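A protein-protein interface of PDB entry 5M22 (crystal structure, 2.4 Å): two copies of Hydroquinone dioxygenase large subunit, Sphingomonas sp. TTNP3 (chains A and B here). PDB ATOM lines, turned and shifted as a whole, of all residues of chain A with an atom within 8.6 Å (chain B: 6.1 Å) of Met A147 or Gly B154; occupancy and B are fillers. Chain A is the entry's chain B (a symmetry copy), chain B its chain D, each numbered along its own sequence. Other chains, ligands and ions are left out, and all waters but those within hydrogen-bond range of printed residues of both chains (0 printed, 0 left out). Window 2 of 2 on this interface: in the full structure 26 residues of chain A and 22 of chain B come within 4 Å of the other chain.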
ATOM      1  N   ASP A 141     -12.955 -10.093  -4.856  1.00  0.00           N
ATOM      2  CA  ASP A 141     -13.756 -11.055  -4.058  1.00  0.00           C
ATOM      3  C   ASP A 141     -14.616 -11.910  -4.992  1.00  0.00           C
ATOM      4  O   ASP A 141     -15.602 -11.416  -5.524  1.00  0.00           O
ATOM      5  CB  ASP A 141     -14.647 -10.302  -3.069  1.00  0.00           C
ATOM      6  CG  ASP A 141     -15.630 -11.231  -2.276  1.00  0.00           C
ATOM      7  OD1 ASP A 141     -15.664 -12.451  -2.559  1.00  0.00           O
ATOM      8  OD2 ASP A 141     -16.363 -10.721  -1.376  1.00  0.00           O
ATOM      9  N   ALA A 144     -18.560 -12.220  -4.529  1.00  0.00           N
ATOM     10  CA  ALA A 144     -19.439 -11.039  -4.668  1.00  0.00           C
ATOM     11  C   ALA A 144     -19.912 -10.834  -6.113  1.00  0.00           C
ATOM     12  O   ALA A 144     -19.364 -11.458  -7.015  1.00  0.00           O
ATOM     13  CB  ALA A 144     -18.728  -9.810  -4.145  1.00  0.00           C
ATOM     14  N   ALA A 145     -20.936 -10.006  -6.324  1.00  0.00           N
ATOM     15  CA  ALA A 145     -21.342  -9.542  -7.684  1.00  0.00           C
ATOM     16  C   ALA A 145     -20.282  -8.624  -8.322  1.00  0.00           C
ATOM     17  O   ALA A 145     -19.516  -7.992  -7.591  1.00  0.00           O
ATOM     18  CB  ALA A 145     -22.676  -8.814  -7.608  1.00  0.00           C
ATOM     19  N   PRO A 146     -20.236  -8.516  -9.675  1.00  0.00           N
ATOM     20  CA  PRO A 146     -19.142  -7.652 -10.236  1.00  0.00           C
ATOM     21  C   PRO A 146     -19.203  -6.171  -9.813  1.00  0.00           C
ATOM     22  O   PRO A 146     -18.165  -5.519  -9.695  1.00  0.00           O
ATOM     23  CB  PRO A 146     -19.298  -7.798 -11.733  1.00  0.00           C
ATOM     24  CG  PRO A 146     -20.025  -9.081 -11.928  1.00  0.00           C
ATOM     25  CD  PRO A 146     -20.875  -9.343 -10.716  1.00  0.00           C
ATOM     26  N   MET A 147     -20.390  -5.645  -9.544  1.00  0.00           N
ATOM     27  CA  MET A 147     -20.491  -4.269  -9.078  1.00  0.00           C
ATOM     28  C   MET A 147     -19.944  -4.028  -7.673  1.00  0.00           C
ATOM     29  O   MET A 147     -19.702  -2.907  -7.298  1.00  0.00           O
ATOM     30  CB  MET A 147     -21.920  -3.736  -9.224  1.00  0.00           C
ATOM     31  CG  MET A 147     -22.261  -3.510 -10.699  1.00  0.00           C
ATOM     32  SD  MET A 147     -23.674  -2.450 -11.043  1.00  0.00           S
ATOM     33  CE  MET A 147     -22.923  -0.836 -10.872  1.00  0.00           C
ATOM     34  N   GLU A 148     -19.725  -5.086  -6.914  1.00  0.00           N
ATOM     35  CA  GLU A 148     -19.362  -4.968  -5.509  1.00  0.00           C
ATOM     36  C   GLU A 148     -17.866  -5.106  -5.220  1.00  0.00           C
ATOM     37  O   GLU A 148     -17.454  -4.923  -4.094  1.00  0.00           O
ATOM     38  CB  GLU A 148     -20.023  -6.096  -4.732  1.00  0.00           C
ATOM     39  CG  GLU A 148     -21.509  -6.246  -4.905  1.00  0.00           C
ATOM     40  CD  GLU A 148     -22.053  -7.223  -3.897  1.00  0.00           C
ATOM     41  OE1 GLU A 148     -22.019  -8.429  -4.155  1.00  0.00           O
ATOM     42  OE2 GLU A 148     -22.491  -6.771  -2.828  1.00  0.00           O
ATOM     43  N   THR A 149     -17.059  -5.506  -6.200  1.00  0.00           N
ATOM     44  CA  THR A 149     -15.671  -5.890  -5.923  1.00  0.00           C
ATOM     45  C   THR A 149     -14.752  -5.475  -7.074  1.00  0.00           C
ATOM     46  O   THR A 149     -15.240  -5.004  -8.086  1.00  0.00           O
ATOM     47  CB  THR A 149     -15.578  -7.398  -5.653  1.00  0.00           C
ATOM     48  OG1 THR A 149     -14.263  -7.683  -5.178  1.00  0.00           O
ATOM     49  CG2 THR A 149     -15.850  -8.231  -6.895  1.00  0.00           C
ATOM     50  N   GLY A 150     -13.440  -5.686  -6.953  1.00  0.00           N
ATOM     51  CA  GLY A 150     -12.482  -5.316  -8.021  1.00  0.00           C
ATOM     52  C   GLY A 150     -12.290  -6.380  -9.102  1.00  0.00           C
ATOM     53  O   GLY A 150     -13.208  -7.144  -9.395  1.00  0.00           O
ATOM     54  N   ARG A 194     -26.362  -2.812   0.065  1.00  0.00           N
ATOM     55  CA  ARG A 194     -26.921  -1.581  -0.522  1.00  0.00           C
ATOM     56  C   ARG A 194     -28.198  -1.842  -1.341  1.00  0.00           C
ATOM     57  O   ARG A 194     -29.086  -0.996  -1.411  1.00  0.00           O
ATOM     58  CB  ARG A 194     -25.876  -0.810  -1.367  1.00  0.00           C
ATOM     59  CG  ARG A 194     -25.633  -1.297  -2.806  1.00  0.00           C
ATOM     60  CD  ARG A 194     -24.813  -2.591  -2.877  1.00  0.00           C
ATOM     61  NE  ARG A 194     -24.418  -2.935  -4.244  1.00  0.00           N
ATOM     62  CZ  ARG A 194     -24.650  -4.101  -4.869  1.00  0.00           C
ATOM     63  NH1 ARG A 194     -24.224  -4.270  -6.112  1.00  0.00           N
ATOM     64  NH2 ARG A 194     -25.290  -5.103  -4.277  1.00  0.00           N
ATOM     65  N   GLN A 195     -28.294  -3.022  -1.947  1.00  0.00           N
ATOM     66  CA  GLN A 195     -29.415  -3.349  -2.816  1.00  0.00           C
ATOM     67  C   GLN A 195     -30.618  -4.033  -2.123  1.00  0.00           C
ATOM     68  O   GLN A 195     -31.508  -4.581  -2.777  1.00  0.00           O
ATOM     69  CB  GLN A 195     -28.915  -4.172  -3.991  1.00  0.00           C
ATOM     70  CG  GLN A 195     -28.108  -3.330  -4.950  1.00  0.00           C
ATOM     71  CD  GLN A 195     -28.171  -3.822  -6.363  1.00  0.00           C
ATOM     72  OE1 GLN A 195     -28.577  -4.956  -6.637  1.00  0.00           O
ATOM     73  NE2 GLN A 195     -27.731  -2.979  -7.286  1.00  0.00           N
ATOM     74  N   GLU A 251     -27.257 -12.288  -7.165  1.00  0.00           N
ATOM     75  CA  GLU A 251     -26.949 -11.104  -7.982  1.00  0.00           C
ATOM     76  C   GLU A 251     -26.067 -11.505  -9.153  1.00  0.00           C
ATOM     77  O   GLU A 251     -25.205 -12.361  -9.025  1.00  0.00           O
ATOM     78  CB  GLU A 251     -26.280 -10.000  -7.145  1.00  0.00           C
ATOM     79  CG  GLU A 251     -26.394  -8.605  -7.764  1.00  0.00           C
ATOM     80  CD  GLU A 251     -25.683  -7.516  -6.967  1.00  0.00           C
ATOM     81  OE1 GLU A 251     -25.705  -7.557  -5.704  1.00  0.00           O
ATOM     82  OE2 GLU A 251     -25.120  -6.596  -7.614  1.00  0.00           O
ATOM     83  N   PHE A 252     -26.319 -10.904 -10.299  1.00  0.00           N
ATOM     84  CA  PHE A 252     -25.635 -11.244 -11.521  1.00  0.00           C
ATOM     85  C   PHE A 252     -25.969 -12.667 -12.056  1.00  0.00           C
ATOM     86  O   PHE A 252     -27.111 -12.917 -12.420  1.00  0.00           O
ATOM     87  CB  PHE A 252     -24.122 -10.930 -11.411  1.00  0.00           C
ATOM     88  CG  PHE A 252     -23.405 -10.968 -12.726  1.00  0.00           C
ATOM     89  CD1 PHE A 252     -23.760 -10.068 -13.771  1.00  0.00           C
ATOM     90  CD2 PHE A 252     -22.400 -11.907 -12.966  1.00  0.00           C
ATOM     91  CE1 PHE A 252     -23.118 -10.113 -15.009  1.00  0.00           C
ATOM     92  CE2 PHE A 252     -21.749 -11.931 -14.210  1.00  0.00           C
ATOM     93  CZ  PHE A 252     -22.109 -11.045 -15.232  1.00  0.00           C
ATOM     94  N   THR A 310     -30.764  -9.419 -12.102  1.00  0.00           N
ATOM     95  CA  THR A 310     -30.324  -8.009 -12.293  1.00  0.00           C
ATOM     96  C   THR A 310     -30.139  -7.244 -10.956  1.00  0.00           C
ATOM     97  O   THR A 310     -29.090  -6.687 -10.666  1.00  0.00           O
ATOM     98  CB  THR A 310     -31.317  -7.215 -13.240  1.00  0.00           C
ATOM     99  OG1 THR A 310     -31.256  -7.714 -14.584  1.00  0.00           O
ATOM    100  CG2 THR A 310     -30.980  -5.748 -13.303  1.00  0.00           C
ATOM    101  N   ARG A 312     -30.160  -7.469  -6.766  1.00  0.00           N
ATOM    102  CA  ARG A 312     -29.837  -8.467  -5.798  1.00  0.00           C
ATOM    103  C   ARG A 312     -31.190  -8.925  -5.301  1.00  0.00           C
ATOM    104  O   ARG A 312     -32.022  -8.103  -4.907  1.00  0.00           O
ATOM    105  CB  ARG A 312     -28.993  -7.880  -4.673  1.00  0.00           C
ATOM    106  CG  ARG A 312     -28.465  -8.909  -3.677  1.00  0.00           C
ATOM    107  CD  ARG A 312     -27.568  -8.226  -2.665  1.00  0.00           C
ATOM    108  NE  ARG A 312     -26.700  -9.095  -1.874  1.00  0.00           N
ATOM    109  CZ  ARG A 312     -25.421  -9.345  -2.170  1.00  0.00           C
ATOM    110  NH1 ARG A 312     -24.857  -8.838  -3.270  1.00  0.00           N
ATOM    111  NH2 ARG A 312     -24.704 -10.117  -1.371  1.00  0.00           N
ATOM    112  N   THR B  30     -33.052   3.098 -15.168  1.00  0.00           N
ATOM    113  CA  THR B  30     -31.809   2.675 -15.823  1.00  0.00           C
ATOM    114  C   THR B  30     -31.147   3.834 -16.556  1.00  0.00           C
ATOM    115  O   THR B  30     -29.927   3.955 -16.542  1.00  0.00           O
ATOM    116  CB  THR B  30     -31.919   1.397 -16.713  1.00  0.00           C
ATOM    117  OG1 THR B  30     -32.611   1.672 -17.925  1.00  0.00           O
ATOM    118  CG2 THR B  30     -32.594   0.269 -15.986  1.00  0.00           C
ATOM    119  N   TYR B  32     -31.306   4.067 -19.738  1.00  0.00           N
ATOM    120  CA  TYR B  32     -31.050   3.542 -21.088  1.00  0.00           C
ATOM    121  C   TYR B  32     -32.293   3.502 -21.977  1.00  0.00           C
ATOM    122  O   TYR B  32     -33.404   3.230 -21.516  1.00  0.00           O
ATOM    123  CB  TYR B  32     -30.446   2.125 -21.015  1.00  0.00           C
ATOM    124  CG  TYR B  32     -29.118   2.033 -20.295  1.00  0.00           C
ATOM    125  CD1 TYR B  32     -27.957   2.567 -20.868  1.00  0.00           C
ATOM    126  CD2 TYR B  32     -29.006   1.391 -19.048  1.00  0.00           C
ATOM    127  CE1 TYR B  32     -26.741   2.472 -20.233  1.00  0.00           C
ATOM    128  CE2 TYR B  32     -27.783   1.292 -18.395  1.00  0.00           C
ATOM    129  CZ  TYR B  32     -26.666   1.838 -19.003  1.00  0.00           C
ATOM    130  OH  TYR B  32     -25.445   1.781 -18.396  1.00  0.00           O
ATOM    131  N   ARG B  44     -31.269  -3.022 -22.163  1.00  0.00           N
ATOM    132  CA  ARG B  44     -30.162  -3.308 -21.262  1.00  0.00           C
ATOM    133  C   ARG B  44     -30.449  -2.720 -19.897  1.00  0.00           C
ATOM    134  O   ARG B  44     -31.102  -1.684 -19.801  1.00  0.00           O
ATOM    135  CB  ARG B  44     -28.824  -2.785 -21.805  1.00  0.00           C
ATOM    136  CG  ARG B  44     -28.568  -1.287 -21.634  1.00  0.00           C
ATOM    137  CD  ARG B  44     -27.102  -0.957 -21.350  1.00  0.00           C
ATOM    138  NE  ARG B  44     -26.681  -1.392 -20.021  1.00  0.00           N
ATOM    139  CZ  ARG B  44     -25.471  -1.175 -19.509  1.00  0.00           C
ATOM    140  NH1 ARG B  44     -24.539  -0.545 -20.235  1.00  0.00           N
ATOM    141  NH2 ARG B  44     -25.187  -1.592 -18.269  1.00  0.00           N
ATOM    142  N   ASP B  45     -29.984  -3.389 -18.840  1.00  0.00           N
ATOM    143  CA  ASP B  45     -30.115  -2.857 -17.520  1.00  0.00           C
ATOM    144  C   ASP B  45     -28.714  -2.763 -16.959  1.00  0.00           C
ATOM    145  O   ASP B  45     -27.775  -2.513 -17.718  1.00  0.00           O
ATOM    146  CB  ASP B  45     -31.004  -3.731 -16.647  1.00  0.00           C
ATOM    147  CG  ASP B  45     -30.640  -5.209 -16.715  1.00  0.00           C
ATOM    148  OD1 ASP B  45     -29.441  -5.543 -16.798  1.00  0.00           O
ATOM    149  OD2 ASP B  45     -31.577  -6.053 -16.675  1.00  0.00           O
ATOM    150  N   GLU B  46     -28.556  -2.982 -15.649  1.00  0.00           N
ATOM    151  CA  GLU B  46     -27.251  -2.777 -15.014  1.00  0.00           C
ATOM    152  C   GLU B  46     -26.183  -3.782 -15.475  1.00  0.00           C
ATOM    153  O   GLU B  46     -25.009  -3.428 -15.517  1.00  0.00           O
ATOM    154  CB  GLU B  46     -27.365  -2.778 -13.472  1.00  0.00           C
ATOM    155  CG  GLU B  46     -28.057  -1.539 -12.890  1.00  0.00           C
ATOM    156  CD  GLU B  46     -29.595  -1.659 -12.835  1.00  0.00           C
ATOM    157  OE1 GLU B  46     -30.207  -2.576 -13.458  1.00  0.00           O
ATOM    158  OE2 GLU B  46     -30.189  -0.817 -12.139  1.00  0.00           O
ATOM    159  N   TYR B  47     -26.593  -4.994 -15.844  1.00  0.00           N
ATOM    160  CA  TYR B  47     -25.672  -6.108 -16.044  1.00  0.00           C
ATOM    161  C   TYR B  47     -25.876  -6.820 -17.361  1.00  0.00           C
ATOM    162  O   TYR B  47     -25.018  -7.597 -17.792  1.00  0.00           O
ATOM    163  CB  TYR B  47     -25.900  -7.188 -14.980  1.00  0.00           C
ATOM    164  CG  TYR B  47     -25.234  -6.967 -13.625  1.00  0.00           C
ATOM    165  CD1 TYR B  47     -23.857  -6.866 -13.520  1.00  0.00           C
ATOM    166  CD2 TYR B  47     -25.998  -6.914 -12.435  1.00  0.00           C
ATOM    167  CE1 TYR B  47     -23.243  -6.680 -12.278  1.00  0.00           C
ATOM    168  CE2 TYR B  47     -25.395  -6.733 -11.199  1.00  0.00           C
ATOM    169  CZ  TYR B  47     -24.016  -6.625 -11.134  1.00  0.00           C
ATOM    170  OH  TYR B  47     -23.392  -6.461  -9.950  1.00  0.00           O
ATOM    171  N   VAL B 137     -21.119   3.709 -22.112  1.00  0.00           N
ATOM    172  CA  VAL B 137     -21.026   4.790 -21.128  1.00  0.00           C
ATOM    173  C   VAL B 137     -19.601   5.409 -21.099  1.00  0.00           C
ATOM    174  O   VAL B 137     -18.677   4.861 -21.715  1.00  0.00           O
ATOM    175  CB  VAL B 137     -21.447   4.287 -19.727  1.00  0.00           C
ATOM    176  CG1 VAL B 137     -22.899   3.821 -19.746  1.00  0.00           C
ATOM    177  CG2 VAL B 137     -20.537   3.150 -19.237  1.00  0.00           C
ATOM    178  N   PRO B 152     -18.622  -1.533 -18.133  1.00  0.00           N
ATOM    179  CA  PRO B 152     -19.883  -1.075 -18.682  1.00  0.00           C
ATOM    180  C   PRO B 152     -21.045  -1.153 -17.694  1.00  0.00           C
ATOM    181  O   PRO B 152     -22.136  -0.668 -18.031  1.00  0.00           O
ATOM    182  CB  PRO B 152     -20.134  -2.088 -19.793  1.00  0.00           C
ATOM    183  CG  PRO B 152     -19.571  -3.366 -19.250  1.00  0.00           C
ATOM    184  CD  PRO B 152     -18.334  -2.940 -18.517  1.00  0.00           C
ATOM    185  N   TRP B 153     -20.840  -1.783 -16.524  1.00  0.00           N
ATOM    186  CA  TRP B 153     -21.928  -2.017 -15.535  1.00  0.00           C
ATOM    187  C   TRP B 153     -22.630  -0.741 -15.070  1.00  0.00           C
ATOM    188  O   TRP B 153     -22.038   0.356 -15.078  1.00  0.00           O
ATOM    189  CB  TRP B 153     -21.477  -2.777 -14.267  1.00  0.00           C
ATOM    190  CG  TRP B 153     -20.458  -3.824 -14.462  1.00  0.00           C
ATOM    191  CD1 TRP B 153     -19.205  -3.817 -13.955  1.00  0.00           C
ATOM    192  CD2 TRP B 153     -20.586  -5.047 -15.209  1.00  0.00           C
ATOM    193  NE1 TRP B 153     -18.526  -4.953 -14.333  1.00  0.00           N
ATOM    194  CE2 TRP B 153     -19.345  -5.725 -15.107  1.00  0.00           C
ATOM    195  CE3 TRP B 153     -21.633  -5.634 -15.959  1.00  0.00           C
ATOM    196  CZ2 TRP B 153     -19.095  -6.955 -15.729  1.00  0.00           C
ATOM    197  CZ3 TRP B 153     -21.402  -6.885 -16.587  1.00  0.00           C
ATOM    198  CH2 TRP B 153     -20.125  -7.535 -16.459  1.00  0.00           C
ATOM    199  N   GLY B 154     -23.896  -0.909 -14.674  1.00  0.00           N
ATOM    200  CA  GLY B 154     -24.628   0.105 -13.927  1.00  0.00           C
ATOM    201  C   GLY B 154     -25.517   0.936 -14.819  1.00  0.00           C
ATOM    202  O   GLY B 154     -25.725   0.599 -15.989  1.00  0.00           O
ATOM    203  N   ILE B 155     -26.021   2.026 -14.248  1.00  0.00           N
ATOM    204  CA  ILE B 155     -26.981   2.894 -14.910  1.00  0.00           C
ATOM    205  C   ILE B 155     -26.304   3.815 -15.930  1.00  0.00           C
ATOM    206  O   ILE B 155     -25.082   4.070 -15.843  1.00  0.00           O
ATOM    207  CB  ILE B 155     -27.778   3.747 -13.892  1.00  0.00           C
ATOM    208  CG1 ILE B 155     -26.835   4.601 -13.038  1.00  0.00           C
ATOM    209  CG2 ILE B 155     -28.704   2.873 -13.029  1.00  0.00           C
ATOM    210  CD1 ILE B 155     -27.414   5.968 -12.752  1.00  0.00           C
ATOM    211  N   LYS B 156     -27.081   4.329 -16.885  1.00  0.00           N
ATOM    212  CA  LYS B 156     -26.491   5.196 -17.907  1.00  0.00           C
ATOM    213  C   LYS B 156     -25.663   6.294 -17.240  1.00  0.00           C
ATOM    214  O   LYS B 156     -26.065   6.856 -16.221  1.00  0.00           O
ATOM    215  CB  LYS B 156     -27.568   5.803 -18.822  1.00  0.00           C
ATOM    216  CG  LYS B 156     -27.074   6.787 -19.898  1.00  0.00           C
ATOM    217  CD  LYS B 156     -26.526   6.119 -21.157  1.00  0.00           C
ATOM    218  CE  LYS B 156     -26.266   7.132 -22.262  1.00  0.00           C
ATOM    219  NZ  LYS B 156     -25.136   6.720 -23.129  1.00  0.00           N
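The side-chain carboxylate (OD2) of Asp B45 sits at hydrogen-bond distance from the side-chain hydroxyl (OG1) of Thr A310 (2.7 Å).
The side-chain hydroxyl (OH) of Tyr B47 lies within hydrogen-bond range of the backbone NH (N) of Met A147 (3.1 Å).
The side-chain hydroxyl of Tyr B47 is in hydrogen-bond range of the side-chain carboxylate of Glu A251 (2.9 Å).
O of Gly B154 is in hydrogen-bond range of OH of Tyr B32 (2.7 Å).
The guanidinium group (NH2) of Arg B44 is in hydrogen-bond range of the backbone carbonyl oxygen (O) of Glu B46.
The side-chain carboxylate (OD1) of Asp B45 is in hydrogen-bond range of the backbone NH (N) of Tyr B47 (3.1 Å).
The backbone carbonyl oxygen (O) of Glu B46 lies within hydrogen-bond range of the backbone NH (N) of Gly B154, at 2.9 Å.
The guanidinium group (NH2) of Arg A194 is in salt-bridge range of the side-chain carboxylate (OE1) of Glu A251 (2.9 Å).
OE1 of Glu A251 is in salt-bridge range of NH1 of Arg A312 (2.9 Å).
Ala A145 touches Tyr B47 (CB to OH, 3.4 Å).
Pro A146 touches Tyr B47.
Pro A146 touches Trp B153.
Met A147 touches Trp B153.
CA of Gly B154 touches CE of Met A147 (3.6 Å).
Phe A252 touches Tyr B47 (CD1 to CD1, 3.2 Å).
Phe A252 touches Trp B153.
OE1 of Glu B46 touches CG2 of Thr A310, 3.3 Å away.
CD2 of Tyr B47 touches O of Thr A310 (3.6 Å).
Printed residues of chain B within 4 Å of Ala A145: Tyr B47.
Of the printed residues of chain B, Pro A146 touches Tyr B47 and Trp B153.
Of the printed residues of chain B, Met A147 touches Tyr B47 (3.1 Å), Trp B153 (3.7 Å) and Gly B154 (3.6 Å).
Thr A149 touches none of the printed residues of chain B.
Of the printed residues of chain A, Glu B46 touches Thr A310 (3.3 Å).
Of the printed residues of chain A, Tyr B47 touches Ala A145 (3.4 Å), Pro A146 (3.8 Å), Met A147 (3.1 Å), Glu A251 (2.9 Å), Phe A252 (3.2 Å) and Thr A310 (3.6 Å).
Of chain A, only Met A147 comes within 4 Å of Gly B154.
The nearest residue of chain B that does not touch Met A147 is Glu B46 (4.4 Å).
The nearest residue of chain A that does not touch Gly B154 is Gln A195 (8.0 Å).
The nearest printed residue of chain A that does not touch Asp B45 is Met A147 (7.8 Å).
Of the 14 printed residues of chain A, 6 touch a printed residue of chain B.
Printed residues of chain A that touch a printed residue of chain B: Ala A145, Pro A146, Met A147, Glu A251, Phe A252 and Thr A310.
Hydrophobic or aromatic side chains of chain A within 4 Å of the printed part of chain B: Ala A145, Pro A146, Met A147 and Phe A252.
Along chain A the printed residues that touch a printed residue of chain B span positions 145 to 310.
Printed residues of chain B that touch a printed residue of chain A: Asp B45, Glu B46, Tyr B47, Trp B153 and Gly B154.
Hydrophobic or aromatic side chains of chain B within 4 Å of the printed part of chain A: Tyr B47 and Trp B153.
Among the printed residues, 12 pairs touch across the chains.
No position is printed for both chains.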
